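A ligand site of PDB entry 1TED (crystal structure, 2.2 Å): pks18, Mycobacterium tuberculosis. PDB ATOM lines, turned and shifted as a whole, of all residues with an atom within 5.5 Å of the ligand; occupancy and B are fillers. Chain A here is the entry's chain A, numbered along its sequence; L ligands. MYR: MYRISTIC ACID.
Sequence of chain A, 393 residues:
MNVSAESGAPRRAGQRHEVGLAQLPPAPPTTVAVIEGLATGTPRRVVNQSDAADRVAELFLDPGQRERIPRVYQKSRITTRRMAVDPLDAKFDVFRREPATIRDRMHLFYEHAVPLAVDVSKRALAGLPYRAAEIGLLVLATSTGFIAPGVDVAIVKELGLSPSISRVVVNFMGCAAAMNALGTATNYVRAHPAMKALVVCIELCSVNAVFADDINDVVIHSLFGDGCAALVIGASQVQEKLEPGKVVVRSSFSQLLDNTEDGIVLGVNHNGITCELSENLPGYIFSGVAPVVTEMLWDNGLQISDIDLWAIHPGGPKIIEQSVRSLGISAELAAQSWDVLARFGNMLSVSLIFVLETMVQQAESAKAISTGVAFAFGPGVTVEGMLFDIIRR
O of His 221 sits close to O2 of the ligand (3.1 Å).
O1 of the ligand is in salt-bridge range of NH2 of Arg 81 (3.9 Å).
The backbone NH of Phe 172 sits close to the side-chain hydroxyl of Ser 143 (3.3 Å).
The guanidinium group of Arg 81 is in hydrogen-bond range of the backbone carbonyl oxygen of His 221 (3.0 Å).
The backbone carbonyl oxygen (O) of His 221 lies within hydrogen-bond range of the side-chain hydroxyl (OH) of Tyr 73 (3.4 Å).
The backbone carbonyl oxygen (O) of Gly 225 sits at hydrogen-bond distance from the side-chain sulfur (SG) of Cys 205 (3.3 Å).
The guanidinium group (NH1) of Arg 81 is in hydrogen-bond range of the backbone carbonyl oxygen (O) of Phe 224.
O of Thr 144 lies close to OD1 of Asn 208 (3.4 Å).
The backbone NH (N) of Ile 273 sits close to the side-chain amide nitrogen (ND2) of Asn 208 (2.7 Å).
The guanidinium group of Arg 81 lies close to the backbone carbonyl oxygen of Ser 222, 3.4 Å away.
Merely in contact with the ligand: Ser 143, Phe 211, Met 83, Pro 87, Cys 205, Phe 224, Ile 220, Thr 144, Ser 206, Cys 275, Asn 208, Ile 273, Leu 348, Tyr 73 and Ala 209.
Hydrophobic or aromatic side chains that line the ligand: Met 83, Pro 87, Phe 211, Ile 220, His 221, Phe 224, Ile 273 and Leu 348.
Within 4 Å of the ligand: Tyr 73, Arg 81, Met 83, Pro 87, Ser 143, Thr 144, Cys 205, Ser 206, Asn 208, Ala 209, Phe 211, Ile 220, His 221, Phe 224, Ile 273, Cys 275 and Leu 348.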
ATOM      1  N   VAL A  47      -4.172 -10.922  -2.863  1.00  0.00           N
ATOM      2  CA  VAL A  47      -4.079 -11.096  -4.310  1.00  0.00           C
ATOM      3  C   VAL A  47      -2.630 -11.030  -4.767  1.00  0.00           C
ATOM      4  O   VAL A  47      -1.945 -10.043  -4.553  1.00  0.00           O
ATOM      5  CB  VAL A  47      -4.889 -10.016  -5.076  1.00  0.00           C
ATOM      6  CG1 VAL A  47      -4.691 -10.193  -6.560  1.00  0.00           C
ATOM      7  CG2 VAL A  47      -6.360 -10.155  -4.752  1.00  0.00           C
ATOM      8  N   ALA A  52      -2.501 -11.916 -10.600  1.00  0.00           N
ATOM      9  CA  ALA A  52      -3.361 -10.826 -11.055  1.00  0.00           C
ATOM     10  C   ALA A  52      -3.055 -10.474 -12.505  1.00  0.00           C
ATOM     11  O   ALA A  52      -3.973 -10.354 -13.328  1.00  0.00           O
ATOM     12  CB  ALA A  52      -3.151  -9.583 -10.174  1.00  0.00           C
ATOM     13  N   VAL A  56      -5.742 -10.844 -15.480  1.00  0.00           N
ATOM     14  CA  VAL A  56      -6.212  -9.625 -16.132  1.00  0.00           C
ATOM     15  C   VAL A  56      -5.859  -9.730 -17.621  1.00  0.00           C
ATOM     16  O   VAL A  56      -6.614  -9.284 -18.482  1.00  0.00           O
ATOM     17  CB  VAL A  56      -5.535  -8.380 -15.539  1.00  0.00           C
ATOM     18  CG1 VAL A  56      -5.887  -7.152 -16.360  1.00  0.00           C
ATOM     19  CG2 VAL A  56      -5.971  -8.205 -14.093  1.00  0.00           C
ATOM     20  N   TYR A  73       2.715  -4.317 -15.299  1.00  0.00           N
ATOM     21  CA  TYR A  73       2.520  -5.127 -14.097  1.00  0.00           C
ATOM     22  C   TYR A  73       3.859  -5.517 -13.507  1.00  0.00           C
ATOM     23  O   TYR A  73       4.030  -5.539 -12.288  1.00  0.00           O
ATOM     24  CB  TYR A  73       1.685  -6.387 -14.401  1.00  0.00           C
ATOM     25  CG  TYR A  73       0.216  -6.240 -14.044  1.00  0.00           C
ATOM     26  CD1 TYR A  73      -0.211  -6.375 -12.717  1.00  0.00           C
ATOM     27  CD2 TYR A  73      -0.730  -5.910 -15.006  1.00  0.00           C
ATOM     28  CE1 TYR A  73      -1.552  -6.181 -12.372  1.00  0.00           C
ATOM     29  CE2 TYR A  73      -2.068  -5.708 -14.673  1.00  0.00           C
ATOM     30  CZ  TYR A  73      -2.463  -5.843 -13.355  1.00  0.00           C
ATOM     31  OH  TYR A  73      -3.778  -5.596 -13.027  1.00  0.00           O
ATOM     32  N   ARG A  81      -1.373  -7.338  -2.614  1.00  0.00           N
ATOM     33  CA  ARG A  81      -2.285  -6.288  -2.157  1.00  0.00           C
ATOM     34  C   ARG A  81      -3.584  -6.961  -1.716  1.00  0.00           C
ATOM     35  O   ARG A  81      -3.930  -8.061  -2.176  1.00  0.00           O
ATOM     36  CB  ARG A  81      -2.514  -5.209  -3.237  1.00  0.00           C
ATOM     37  CG  ARG A  81      -2.682  -5.722  -4.628  1.00  0.00           C
ATOM     38  CD  ARG A  81      -2.754  -4.587  -5.659  1.00  0.00           C
ATOM     39  NE  ARG A  81      -2.739  -5.145  -7.008  1.00  0.00           N
ATOM     40  CZ  ARG A  81      -3.423  -4.666  -8.032  1.00  0.00           C
ATOM     41  NH1 ARG A  81      -4.180  -3.582  -7.888  1.00  0.00           N
ATOM     42  NH2 ARG A  81      -3.359  -5.269  -9.211  1.00  0.00           N
ATOM     43  N   MET A  83      -7.815  -7.154  -0.979  1.00  0.00           N
ATOM     44  CA  MET A  83      -9.058  -6.718  -1.582  1.00  0.00           C
ATOM     45  C   MET A  83     -10.287  -7.296  -0.889  1.00  0.00           C
ATOM     46  O   MET A  83     -10.378  -8.505  -0.650  1.00  0.00           O
ATOM     47  CB  MET A  83      -9.061  -7.068  -3.060  1.00  0.00           C
ATOM     48  CG  MET A  83      -7.905  -6.426  -3.814  1.00  0.00           C
ATOM     49  SD  MET A  83      -7.940  -6.770  -5.566  1.00  0.00           S
ATOM     50  CE  MET A  83      -6.277  -6.224  -6.060  1.00  0.00           C
ATOM     51  N   PRO A  87     -12.441  -8.687  -7.788  1.00  0.00           N
ATOM     52  CA  PRO A  87     -12.923  -8.137  -9.058  1.00  0.00           C
ATOM     53  C   PRO A  87     -13.110  -9.127 -10.214  1.00  0.00           C
ATOM     54  O   PRO A  87     -14.026  -8.995 -11.018  1.00  0.00           O
ATOM     55  CB  PRO A  87     -11.896  -7.048  -9.362  1.00  0.00           C
ATOM     56  CG  PRO A  87     -10.641  -7.588  -8.734  1.00  0.00           C
ATOM     57  CD  PRO A  87     -11.152  -8.077  -7.414  1.00  0.00           C
ATOM     58  N   SER A 143     -12.043   8.220  -0.499  1.00  0.00           N
ATOM     59  CA  SER A 143     -12.208   8.735  -1.854  1.00  0.00           C
ATOM     60  C   SER A 143     -12.774   7.605  -2.701  1.00  0.00           C
ATOM     61  O   SER A 143     -12.849   7.715  -3.919  1.00  0.00           O
ATOM     62  CB  SER A 143     -10.869   9.215  -2.410  1.00  0.00           C
ATOM     63  OG  SER A 143     -10.466  10.417  -1.770  1.00  0.00           O
ATOM     64  N   THR A 144     -13.200   6.529  -2.047  1.00  0.00           N
ATOM     65  CA  THR A 144     -13.736   5.357  -2.746  1.00  0.00           C
ATOM     66  C   THR A 144     -15.124   4.898  -2.296  1.00  0.00           C
ATOM     67  O   THR A 144     -15.565   3.815  -2.660  1.00  0.00           O
ATOM     68  CB  THR A 144     -12.772   4.148  -2.604  1.00  0.00           C
ATOM     69  OG1 THR A 144     -12.425   3.974  -1.217  1.00  0.00           O
ATOM     70  CG2 THR A 144     -11.494   4.373  -3.421  1.00  0.00           C
ATOM     71  N   PHE A 172     -12.739  12.788  -1.271  1.00  0.00           N
ATOM     72  CA  PHE A 172     -11.999  13.242  -2.448  1.00  0.00           C
ATOM     73  C   PHE A 172     -10.761  14.113  -2.272  1.00  0.00           C
ATOM     74  O   PHE A 172     -10.456  14.958  -3.121  1.00  0.00           O
ATOM     75  CB  PHE A 172     -12.964  13.918  -3.437  1.00  0.00           C
ATOM     76  CG  PHE A 172     -13.460  12.991  -4.521  1.00  0.00           C
ATOM     77  CD1 PHE A 172     -13.307  11.615  -4.403  1.00  0.00           C
ATOM     78  CD2 PHE A 172     -14.086  13.503  -5.659  1.00  0.00           C
ATOM     79  CE1 PHE A 172     -13.759  10.759  -5.404  1.00  0.00           C
ATOM     80  CE2 PHE A 172     -14.545  12.659  -6.662  1.00  0.00           C
ATOM     81  CZ  PHE A 172     -14.373  11.279  -6.533  1.00  0.00           C
ATOM     82  N   CYS A 205     -10.677   0.296  -2.962  1.00  0.00           N
ATOM     83  CA  CYS A 205     -10.563   0.430  -4.410  1.00  0.00           C
ATOM     84  C   CYS A 205     -11.192  -0.754  -5.161  1.00  0.00           C
ATOM     85  O   CYS A 205     -11.899  -0.546  -6.150  1.00  0.00           O
ATOM     86  CB  CYS A 205      -9.091   0.560  -4.803  1.00  0.00           C
ATOM     87  SG  CYS A 205      -8.232   2.033  -4.154  1.00  0.00           S
ATOM     88  N   SER A 206     -10.937  -1.967  -4.688  1.00  0.00           N
ATOM     89  CA  SER A 206     -11.446  -3.181  -5.330  1.00  0.00           C
ATOM     90  C   SER A 206     -12.933  -3.083  -5.654  1.00  0.00           C
ATOM     91  O   SER A 206     -13.426  -3.691  -6.598  1.00  0.00           O
ATOM     92  CB  SER A 206     -11.184  -4.418  -4.440  1.00  0.00           C
ATOM     93  OG  SER A 206     -11.961  -4.421  -3.254  1.00  0.00           O
ATOM     94  N   ASN A 208     -14.425  -0.581  -6.832  1.00  0.00           N
ATOM     95  CA  ASN A 208     -14.667   0.225  -8.028  1.00  0.00           C
ATOM     96  C   ASN A 208     -14.029  -0.347  -9.283  1.00  0.00           C
ATOM     97  O   ASN A 208     -13.935   0.325 -10.308  1.00  0.00           O
ATOM     98  CB  ASN A 208     -14.160   1.668  -7.820  1.00  0.00           C
ATOM     99  CG  ASN A 208     -14.937   2.414  -6.733  1.00  0.00           C
ATOM    100  OD1 ASN A 208     -14.568   2.386  -5.557  1.00  0.00           O
ATOM    101  ND2 ASN A 208     -16.020   3.072  -7.128  1.00  0.00           N
ATOM    102  N   ALA A 209     -13.593  -1.609  -9.222  1.00  0.00           N
ATOM    103  CA  ALA A 209     -12.975  -2.268 -10.376  1.00  0.00           C
ATOM    104  C   ALA A 209     -13.863  -2.220 -11.623  1.00  0.00           C
ATOM    105  O   ALA A 209     -15.072  -2.494 -11.554  1.00  0.00           O
ATOM    106  CB  ALA A 209     -12.647  -3.706 -10.033  1.00  0.00           C
ATOM    107  N   VAL A 210     -13.281  -1.885 -12.769  1.00  0.00           N
ATOM    108  CA  VAL A 210     -14.035  -1.800 -14.006  1.00  0.00           C
ATOM    109  C   VAL A 210     -13.294  -2.433 -15.189  1.00  0.00           C
ATOM    110  O   VAL A 210     -13.916  -3.011 -16.091  1.00  0.00           O
ATOM    111  CB  VAL A 210     -14.363  -0.319 -14.335  1.00  0.00           C
ATOM    112  CG1 VAL A 210     -14.966  -0.208 -15.711  1.00  0.00           C
ATOM    113  CG2 VAL A 210     -15.354   0.228 -13.319  1.00  0.00           C
ATOM    114  N   PHE A 211     -11.970  -2.328 -15.181  1.00  0.00           N
ATOM    115  CA  PHE A 211     -11.104  -2.884 -16.219  1.00  0.00           C
ATOM    116  C   PHE A 211     -11.390  -2.287 -17.600  1.00  0.00           C
ATOM    117  O   PHE A 211     -11.824  -2.980 -18.511  1.00  0.00           O
ATOM    118  CB  PHE A 211     -11.239  -4.407 -16.253  1.00  0.00           C
ATOM    119  CG  PHE A 211     -10.781  -5.087 -14.987  1.00  0.00           C
ATOM    120  CD1 PHE A 211      -9.427  -5.272 -14.727  1.00  0.00           C
ATOM    121  CD2 PHE A 211     -11.708  -5.518 -14.041  1.00  0.00           C
ATOM    122  CE1 PHE A 211      -9.006  -5.878 -13.542  1.00  0.00           C
ATOM    123  CE2 PHE A 211     -11.287  -6.123 -12.846  1.00  0.00           C
ATOM    124  CZ  PHE A 211      -9.929  -6.301 -12.607  1.00  0.00           C
ATOM    125  N   ILE A 220      -3.971   2.025 -12.999  1.00  0.00           N
ATOM    126  CA  ILE A 220      -4.654   2.164 -11.717  1.00  0.00           C
ATOM    127  C   ILE A 220      -5.050   0.783 -11.182  1.00  0.00           C
ATOM    128  O   ILE A 220      -4.868   0.483  -9.996  1.00  0.00           O
ATOM    129  CB  ILE A 220      -5.919   3.058 -11.877  1.00  0.00           C
ATOM    130  CG1 ILE A 220      -5.678   4.403 -11.190  1.00  0.00           C
ATOM    131  CG2 ILE A 220      -7.132   2.385 -11.322  1.00  0.00           C
ATOM    132  CD1 ILE A 220      -4.629   5.242 -11.864  1.00  0.00           C
ATOM    133  N   HIS A 221      -5.568  -0.060 -12.056  1.00  0.00           N
ATOM    134  CA  HIS A 221      -5.992  -1.388 -11.661  1.00  0.00           C
ATOM    135  C   HIS A 221      -4.832  -2.314 -11.318  1.00  0.00           C
ATOM    136  O   HIS A 221      -5.031  -3.379 -10.749  1.00  0.00           O
ATOM    137  CB  HIS A 221      -6.864  -2.014 -12.746  1.00  0.00           C
ATOM    138  CG  HIS A 221      -8.250  -1.429 -12.798  1.00  0.00           C
ATOM    139  ND1 HIS A 221      -9.380  -2.207 -12.660  1.00  0.00           N
ATOM    140  CD2 HIS A 221      -8.676  -0.165 -12.990  1.00  0.00           C
ATOM    141  CE1 HIS A 221     -10.452  -1.433 -12.768  1.00  0.00           C
ATOM    142  NE2 HIS A 221     -10.054  -0.188 -12.961  1.00  0.00           N
ATOM    143  N   SER A 222      -3.618  -1.898 -11.667  1.00  0.00           N
ATOM    144  CA  SER A 222      -2.459  -2.723 -11.358  1.00  0.00           C
ATOM    145  C   SER A 222      -1.802  -2.192 -10.086  1.00  0.00           C
ATOM    146  O   SER A 222      -0.979  -2.876  -9.473  1.00  0.00           O
ATOM    147  CB  SER A 222      -1.438  -2.688 -12.511  1.00  0.00           C
ATOM    148  OG  SER A 222      -0.638  -1.515 -12.480  1.00  0.00           O
ATOM    149  N   PHE A 224      -3.705   0.098  -7.404  1.00  0.00           N
ATOM    150  CA  PHE A 224      -4.583   0.325  -6.262  1.00  0.00           C
ATOM    151  C   PHE A 224      -5.048  -0.900  -5.467  1.00  0.00           C
ATOM    152  O   PHE A 224      -5.412  -1.934  -6.018  1.00  0.00           O
ATOM    153  CB  PHE A 224      -5.780   1.161  -6.734  1.00  0.00           C
ATOM    154  CG  PHE A 224      -5.410   2.533  -7.228  1.00  0.00           C
ATOM    155  CD1 PHE A 224      -4.078   2.878  -7.463  1.00  0.00           C
ATOM    156  CD2 PHE A 224      -6.382   3.494  -7.458  1.00  0.00           C
ATOM    157  CE1 PHE A 224      -3.716   4.154  -7.914  1.00  0.00           C
ATOM    158  CE2 PHE A 224      -6.037   4.784  -7.912  1.00  0.00           C
ATOM    159  CZ  PHE A 224      -4.710   5.111  -8.134  1.00  0.00           C
ATOM    160  N   GLY A 225      -5.006  -0.757  -4.143  1.00  0.00           N
ATOM    161  CA  GLY A 225      -5.407  -1.831  -3.245  1.00  0.00           C
ATOM    162  C   GLY A 225      -6.355  -1.340  -2.161  1.00  0.00           C
ATOM    163  O   GLY A 225      -6.762  -0.183  -2.156  1.00  0.00           O
ATOM    164  N   LEU A 266      -9.889  13.094  -9.799  1.00  0.00           N
ATOM    165  CA  LEU A 266     -10.819  12.125  -9.236  1.00  0.00           C
ATOM    166  C   LEU A 266     -12.216  12.437  -9.746  1.00  0.00           C
ATOM    167  O   LEU A 266     -12.581  13.597  -9.882  1.00  0.00           O
ATOM    168  CB  LEU A 266     -10.806  12.176  -7.708  1.00  0.00           C
ATOM    169  CG  LEU A 266      -9.424  11.999  -7.064  1.00  0.00           C
ATOM    170  CD1 LEU A 266      -9.562  11.988  -5.533  1.00  0.00           C
ATOM    171  CD2 LEU A 266      -8.792  10.708  -7.558  1.00  0.00           C
ATOM    172  N   ILE A 273     -16.093   4.937  -9.095  1.00  0.00           N
ATOM    173  CA  ILE A 273     -15.220   6.079  -8.896  1.00  0.00           C
ATOM    174  C   ILE A 273     -13.922   5.746  -9.617  1.00  0.00           C
ATOM    175  O   ILE A 273     -13.541   4.583  -9.722  1.00  0.00           O
ATOM    176  CB  ILE A 273     -14.937   6.312  -7.404  1.00  0.00           C
ATOM    177  CG1 ILE A 273     -16.234   6.727  -6.693  1.00  0.00           C
ATOM    178  CG2 ILE A 273     -13.856   7.370  -7.247  1.00  0.00           C
ATOM    179  CD1 ILE A 273     -16.121   6.716  -5.184  1.00  0.00           C
ATOM    180  N   THR A 274     -13.250   6.772 -10.125  1.00  0.00           N
ATOM    181  CA  THR A 274     -12.017   6.584 -10.838  1.00  0.00           C
ATOM    182  C   THR A 274     -11.008   7.682 -10.517  1.00  0.00           C
ATOM    183  O   THR A 274     -11.361   8.716  -9.960  1.00  0.00           O
ATOM    184  CB  THR A 274     -12.283   6.562 -12.357  1.00  0.00           C
ATOM    185  OG1 THR A 274     -11.117   6.094 -13.035  1.00  0.00           O
ATOM    186  CG2 THR A 274     -12.631   7.967 -12.838  1.00  0.00           C
ATOM    187  N   CYS A 275      -9.755   7.428 -10.877  1.00  0.00           N
ATOM    188  CA  CYS A 275      -8.672   8.388 -10.667  1.00  0.00           C
ATOM    189  C   CYS A 275      -7.878   8.467 -11.964  1.00  0.00           C
ATOM    190  O   CYS A 275      -7.420   7.451 -12.480  1.00  0.00           O
ATOM    191  CB  CYS A 275      -7.761   7.933  -9.527  1.00  0.00           C
ATOM    192  SG  CYS A 275      -6.203   8.869  -9.380  1.00  0.00           S
ATOM    193  N   LEU A 348      -4.237   4.494  -1.204  1.00  0.00           N
ATOM    194  CA  LEU A 348      -4.594   5.902  -1.090  1.00  0.00           C
ATOM    195  C   LEU A 348      -4.232   6.514   0.264  1.00  0.00           C
ATOM    196  O   LEU A 348      -3.103   6.355   0.735  1.00  0.00           O
ATOM    197  CB  LEU A 348      -6.100   6.050  -1.400  1.00  0.00           C
ATOM    198  CG  LEU A 348      -6.482   6.063  -2.898  1.00  0.00           C
ATOM    199  CD1 LEU A 348      -5.645   5.078  -3.669  1.00  0.00           C
ATOM    200  CD2 LEU A 348      -7.948   5.737  -3.064  1.00  0.00           C
HETATM  201  C1  MYR L   1      -7.514  -5.799  -9.840  1.00  0.00           C
HETATM  202  O1  MYR L   1      -6.980  -6.766  -9.291  1.00  0.00           O
HETATM  203  O2  MYR L   1      -7.209  -5.537 -11.006  1.00  0.00           O
HETATM  204  C2  MYR L   1      -8.539  -4.943  -9.099  1.00  0.00           C
HETATM  205  C3  MYR L   1      -7.984  -3.537  -8.825  1.00  0.00           C
HETATM  206  C4  MYR L   1      -9.003  -2.689  -8.052  1.00  0.00           C
HETATM  207  C5  MYR L   1      -8.473  -1.271  -7.820  1.00  0.00           C
HETATM  208  C6  MYR L   1      -8.309  -0.486  -9.130  1.00  0.00           C
HETATM  209  C7  MYR L   1      -9.646  -0.147  -9.794  1.00  0.00           C
HETATM  210  C8  MYR L   1     -10.460   0.858  -8.975  1.00  0.00           C
HETATM  211  C9  MYR L   1      -9.755   2.202  -8.869  1.00  0.00           C
HETATM  212  C10 MYR L   1     -10.511   3.144  -7.929  1.00  0.00           C
HETATM  213  C11 MYR L   1      -9.771   4.475  -7.769  1.00  0.00           C
HETATM  214  C12 MYR L   1     -10.505   5.395  -6.785  1.00  0.00           C
HETATM  215  C13 MYR L   1      -9.707   6.684  -6.578  1.00  0.00           C
HETATM  216  C14 MYR L   1     -10.400   7.606  -5.572  1.00  0.00           C
